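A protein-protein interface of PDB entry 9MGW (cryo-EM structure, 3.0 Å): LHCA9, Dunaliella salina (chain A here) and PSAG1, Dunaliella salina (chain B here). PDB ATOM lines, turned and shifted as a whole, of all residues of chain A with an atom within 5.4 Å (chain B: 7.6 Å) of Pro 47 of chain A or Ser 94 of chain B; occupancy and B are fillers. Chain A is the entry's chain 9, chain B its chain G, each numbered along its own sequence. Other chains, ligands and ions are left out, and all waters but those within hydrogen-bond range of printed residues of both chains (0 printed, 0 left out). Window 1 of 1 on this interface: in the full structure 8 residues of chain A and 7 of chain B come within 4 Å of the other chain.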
ATOM      1  N   ILE A  44       9.347 -12.666  -5.843  1.00  0.00           N
ATOM      2  CA  ILE A  44       8.569 -12.147  -4.722  1.00  0.00           C
ATOM      3  C   ILE A  44       7.345 -13.043  -4.565  1.00  0.00           C
ATOM      4  O   ILE A  44       6.627 -13.260  -5.554  1.00  0.00           O
ATOM      5  CB  ILE A  44       8.168 -10.677  -4.937  1.00  0.00           C
ATOM      6  CG1 ILE A  44       9.208  -9.731  -4.330  1.00  0.00           C
ATOM      7  CG2 ILE A  44       6.824 -10.360  -4.285  1.00  0.00           C
ATOM      8  CD1 ILE A  44      10.526  -9.672  -5.069  1.00  0.00           C
ATOM      9  N   PRO A  45       7.154 -13.680  -3.417  1.00  0.00           N
ATOM     10  CA  PRO A  45       5.851 -14.277  -3.085  1.00  0.00           C
ATOM     11  C   PRO A  45       4.936 -13.258  -2.425  1.00  0.00           C
ATOM     12  O   PRO A  45       4.933 -13.141  -1.190  1.00  0.00           O
ATOM     13  CB  PRO A  45       6.218 -15.415  -2.122  1.00  0.00           C
ATOM     14  CG  PRO A  45       7.514 -14.993  -1.503  1.00  0.00           C
ATOM     15  CD  PRO A  45       8.204 -14.043  -2.447  1.00  0.00           C
ATOM     16  N   PRO A  46       4.176 -12.485  -3.202  1.00  0.00           N
ATOM     17  CA  PRO A  46       3.407 -11.372  -2.625  1.00  0.00           C
ATOM     18  C   PRO A  46       2.335 -11.880  -1.678  1.00  0.00           C
ATOM     19  O   PRO A  46       1.649 -12.871  -1.973  1.00  0.00           O
ATOM     20  CB  PRO A  46       2.785 -10.688  -3.854  1.00  0.00           C
ATOM     21  CG  PRO A  46       3.247 -11.479  -5.061  1.00  0.00           C
ATOM     22  CD  PRO A  46       3.703 -12.806  -4.556  1.00  0.00           C
ATOM     23  N   PRO A  47       2.160 -11.230  -0.527  1.00  0.00           N
ATOM     24  CA  PRO A  47       1.292 -11.794   0.516  1.00  0.00           C
ATOM     25  C   PRO A  47      -0.191 -11.685   0.200  1.00  0.00           C
ATOM     26  O   PRO A  47      -0.948 -12.633   0.436  1.00  0.00           O
ATOM     27  CB  PRO A  47       1.658 -10.982   1.767  1.00  0.00           C
ATOM     28  CG  PRO A  47       2.536  -9.846   1.305  1.00  0.00           C
ATOM     29  CD  PRO A  47       2.661  -9.889  -0.183  1.00  0.00           C
ATOM     30  N   HIS A  48      -0.620 -10.545  -0.333  1.00  0.00           N
ATOM     31  CA  HIS A  48      -2.042 -10.312  -0.548  1.00  0.00           C
ATOM     32  C   HIS A  48      -2.487 -10.592  -1.976  1.00  0.00           C
ATOM     33  O   HIS A  48      -3.650 -10.950  -2.193  1.00  0.00           O
ATOM     34  CB  HIS A  48      -2.404  -8.871  -0.177  1.00  0.00           C
ATOM     35  CG  HIS A  48      -3.871  -8.656   0.022  1.00  0.00           C
ATOM     36  ND1 HIS A  48      -4.520  -7.514  -0.398  1.00  0.00           N
ATOM     37  CD2 HIS A  48      -4.816  -9.436   0.597  1.00  0.00           C
ATOM     38  CE1 HIS A  48      -5.802  -7.602  -0.091  1.00  0.00           C
ATOM     39  NE2 HIS A  48      -6.008  -8.757   0.514  1.00  0.00           N
ATOM     40  N   LEU A  49      -1.598 -10.437  -2.953  1.00  0.00           N
ATOM     41  CA  LEU A  49      -1.946 -10.611  -4.362  1.00  0.00           C
ATOM     42  C   LEU A  49      -1.619 -12.047  -4.765  1.00  0.00           C
ATOM     43  O   LEU A  49      -0.467 -12.374  -5.063  1.00  0.00           O
ATOM     44  CB  LEU A  49      -1.205  -9.597  -5.227  1.00  0.00           C
ATOM     45  CG  LEU A  49      -1.327  -8.149  -4.750  1.00  0.00           C
ATOM     46  CD1 LEU A  49      -0.466  -7.220  -5.592  1.00  0.00           C
ATOM     47  CD2 LEU A  49      -2.780  -7.698  -4.755  1.00  0.00           C
ATOM     48  N   GLY A  58       1.861  -8.522  -8.760  1.00  0.00           N
ATOM     49  CA  GLY A  58       2.509  -8.426  -7.470  1.00  0.00           C
ATOM     50  C   GLY A  58       3.192  -7.107  -7.199  1.00  0.00           C
ATOM     51  O   GLY A  58       4.053  -7.036  -6.315  1.00  0.00           O
ATOM     52  N   ASP A  60       3.441  -4.164  -5.439  1.00  0.00           N
ATOM     53  CA  ASP A  60       3.035  -3.445  -4.239  1.00  0.00           C
ATOM     54  C   ASP A  60       4.214  -3.353  -3.277  1.00  0.00           C
ATOM     55  O   ASP A  60       4.262  -4.091  -2.285  1.00  0.00           O
ATOM     56  CB  ASP A  60       1.846  -4.129  -3.563  1.00  0.00           C
ATOM     57  CG  ASP A  60       0.864  -3.138  -2.967  1.00  0.00           C
ATOM     58  OD1 ASP A  60       1.279  -2.001  -2.659  1.00  0.00           O
ATOM     59  OD2 ASP A  60      -0.321  -3.495  -2.805  1.00  0.00           O
ATOM     60  N   PRO A  61       5.182  -2.466  -3.531  1.00  0.00           N
ATOM     61  CA  PRO A  61       6.346  -2.371  -2.634  1.00  0.00           C
ATOM     62  C   PRO A  61       6.040  -1.731  -1.291  1.00  0.00           C
ATOM     63  O   PRO A  61       6.902  -1.768  -0.404  1.00  0.00           O
ATOM     64  CB  PRO A  61       7.335  -1.518  -3.436  1.00  0.00           C
ATOM     65  CG  PRO A  61       6.472  -0.687  -4.316  1.00  0.00           C
ATOM     66  CD  PRO A  61       5.298  -1.551  -4.680  1.00  0.00           C
ATOM     67  N   LYS B  91       3.832  -3.477   8.960  1.00  0.00           N
ATOM     68  CA  LYS B  91       4.553  -4.708   8.696  1.00  0.00           C
ATOM     69  C   LYS B  91       5.597  -4.475   7.605  1.00  0.00           C
ATOM     70  O   LYS B  91       5.440  -3.576   6.772  1.00  0.00           O
ATOM     71  CB  LYS B  91       3.580  -5.810   8.274  1.00  0.00           C
ATOM     72  CG  LYS B  91       2.585  -6.201   9.351  1.00  0.00           C
ATOM     73  CD  LYS B  91       3.289  -6.619  10.630  1.00  0.00           C
ATOM     74  CE  LYS B  91       3.201  -8.121  10.846  1.00  0.00           C
ATOM     75  NZ  LYS B  91       3.971  -8.551  12.044  1.00  0.00           N
ATOM     76  N   PRO B  92       6.684  -5.254   7.597  1.00  0.00           N
ATOM     77  CA  PRO B  92       7.713  -5.066   6.566  1.00  0.00           C
ATOM     78  C   PRO B  92       7.188  -5.384   5.173  1.00  0.00           C
ATOM     79  O   PRO B  92       6.260  -6.176   4.997  1.00  0.00           O
ATOM     80  CB  PRO B  92       8.821  -6.041   6.984  1.00  0.00           C
ATOM     81  CG  PRO B  92       8.139  -7.050   7.838  1.00  0.00           C
ATOM     82  CD  PRO B  92       7.079  -6.286   8.571  1.00  0.00           C
ATOM     83  N   ALA B  93       7.796  -4.739   4.178  1.00  0.00           N
ATOM     84  CA  ALA B  93       7.372  -4.878   2.794  1.00  0.00           C
ATOM     85  C   ALA B  93       7.659  -6.284   2.274  1.00  0.00           C
ATOM     86  O   ALA B  93       8.272  -7.111   2.947  1.00  0.00           O
ATOM     87  CB  ALA B  93       8.071  -3.842   1.913  1.00  0.00           C
ATOM     88  N   SER B  94       7.194  -6.549   1.052  1.00  0.00           N
ATOM     89  CA  SER B  94       7.312  -7.894   0.500  1.00  0.00           C
ATOM     90  C   SER B  94       8.598  -8.079  -0.296  1.00  0.00           C
ATOM     91  O   SER B  94       9.008  -9.217  -0.549  1.00  0.00           O
ATOM     92  CB  SER B  94       6.103  -8.210  -0.380  1.00  0.00           C
ATOM     93  OG  SER B  94       6.228  -7.597  -1.652  1.00  0.00           O
ATOM     94  N   PHE B  95       9.247  -6.989  -0.700  1.00  0.00           N
ATOM     95  CA  PHE B  95      10.395  -7.064  -1.594  1.00  0.00           C
ATOM     96  C   PHE B  95      11.726  -6.785  -0.905  1.00  0.00           C
ATOM     97  O   PHE B  95      12.748  -6.682  -1.589  1.00  0.00           O
ATOM     98  CB  PHE B  95      10.209  -6.094  -2.769  1.00  0.00           C
ATOM     99  CG  PHE B  95      10.546  -4.662  -2.445  1.00  0.00           C
ATOM    100  CD1 PHE B  95       9.751  -3.923  -1.584  1.00  0.00           C
ATOM    101  CD2 PHE B  95      11.653  -4.052  -3.014  1.00  0.00           C
ATOM    102  CE1 PHE B  95      10.058  -2.608  -1.287  1.00  0.00           C
ATOM    103  CE2 PHE B  95      11.967  -2.736  -2.722  1.00  0.00           C
ATOM    104  CZ  PHE B  95      11.169  -2.015  -1.857  1.00  0.00           C
ATOM    105  N   VAL B  96      11.752  -6.678   0.426  1.00  0.00           N
ATOM    106  CA  VAL B  96      12.972  -6.308   1.134  1.00  0.00           C
ATOM    107  C   VAL B  96      13.571  -7.459   1.926  1.00  0.00           C
ATOM    108  O   VAL B  96      14.618  -7.274   2.562  1.00  0.00           O
ATOM    109  CB  VAL B  96      12.729  -5.100   2.062  1.00  0.00           C
ATOM    110  CG1 VAL B  96      12.309  -3.886   1.252  1.00  0.00           C
ATOM    111  CG2 VAL B  96      11.679  -5.435   3.107  1.00  0.00           C
ATOM    112  N   GLU B  97      12.958  -8.647   1.901  1.00  0.00           N
ATOM    113  CA  GLU B  97      13.469  -9.752   2.708  1.00  0.00           C
ATOM    114  C   GLU B  97      13.439 -11.076   1.950  1.00  0.00           C
ATOM    115  O   GLU B  97      13.553 -12.142   2.567  1.00  0.00           O
ATOM    116  CB  GLU B  97      12.677  -9.906   4.017  1.00  0.00           C
ATOM    117  CG  GLU B  97      11.202 -10.394   3.925  1.00  0.00           C
ATOM    118  CD  GLU B  97      10.230  -9.528   3.120  1.00  0.00           C
ATOM    119  OE1 GLU B  97       9.024  -9.848   3.154  1.00  0.00           O
ATOM    120  OE2 GLU B  97      10.631  -8.535   2.479  1.00  0.00           O
ATOM    121  N   THR B  98      13.267 -11.029   0.627  1.00  0.00           N
ATOM    122  CA  THR B  98      13.080 -12.244  -0.164  1.00  0.00           C
ATOM    123  C   THR B  98      14.315 -13.139  -0.132  1.00  0.00           C
ATOM    124  O   THR B  98      14.291 -14.219   0.465  1.00  0.00           O
ATOM    125  CB  THR B  98      12.731 -11.878  -1.606  1.00  0.00           C
ATOM    126  OG1 THR B  98      13.699 -10.949  -2.107  1.00  0.00           O
ATOM    127  CG2 THR B  98      11.361 -11.237  -1.664  1.00  0.00           C
ATOM    128  N   LYS B  99      15.402 -12.691  -0.752  1.00  0.00           N
ATOM    129  CA  LYS B  99      16.708 -13.353  -0.728  1.00  0.00           C
ATOM    130  C   LYS B  99      17.714 -12.369  -1.312  1.00  0.00           C
ATOM    131  O   LYS B  99      17.382 -11.209  -1.589  1.00  0.00           O
ATOM    132  CB  LYS B  99      16.686 -14.701  -1.467  1.00  0.00           C
ATOM    133  CG  LYS B  99      16.339 -14.676  -2.959  1.00  0.00           C
ATOM    134  CD  LYS B  99      17.240 -15.586  -3.811  1.00  0.00           C
ATOM    135  CE  LYS B  99      18.360 -14.821  -4.496  1.00  0.00           C
ATOM    136  NZ  LYS B  99      19.131 -15.663  -5.448  1.00  0.00           N
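Among the printed residues, pairs that only touch across the chains: Pro 61 of chain A with Ala 93 of chain B (3.3 Å), Pro 61 of chain A with Phe 95 of chain B (3.4 Å), Ile 44 of chain A with Thr 98 of chain B (3.7 Å), Ile 44 of chain A with Ser 94 of chain B (3.8 Å) and Pro 47 of chain A with Ser 94 of chain B (3.8 Å).
Of chain B, only Ser 94 comes within 4 Å of Pro 47 of chain A.
Ser 94 of chain B touches just these residues of chain A: Ile 44 (3.8 Å) and Pro 47 (3.8 Å).
Printed residues of chain A within 4 Å of Thr 98 of chain B: Ile 44 (3.7 Å).
Of the printed residues of chain B, Pro 61 of chain A touches Ala 93 and Phe 95.
Of the printed residues of chain B, Ile 44 of chain A touches Ser 94 (3.8 Å) and Thr 98 (3.7 Å).
Of the printed residues of chain A, Ala 93 of chain B touches Pro 61 (3.3 Å).
Gly 58 of chain A touches none of the printed residues of chain B.
Pro 46 of chain A touches none of the printed residues of chain B.
The nearest residue of chain B that does not touch Pro 47 of chain A is Ala 93 of chain B (6.3 Å).
Printed residues of chain A that touch a printed residue of chain B: Ile 44, Pro 47 and Pro 61.
Of the 9 printed residues of chain B, 4 touch a printed residue of chain A.
Printed residues of chain B that touch a printed residue of chain A: Ala 93, Ser 94, Phe 95 and Thr 98.
Along chain B the printed residues that touch a printed residue of chain A span positions 93 to 98.
Among the printed residues, no Asp or Glu carboxylate lies within 4 Å of a Lys or Arg side-chain nitrogen of the other chain.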
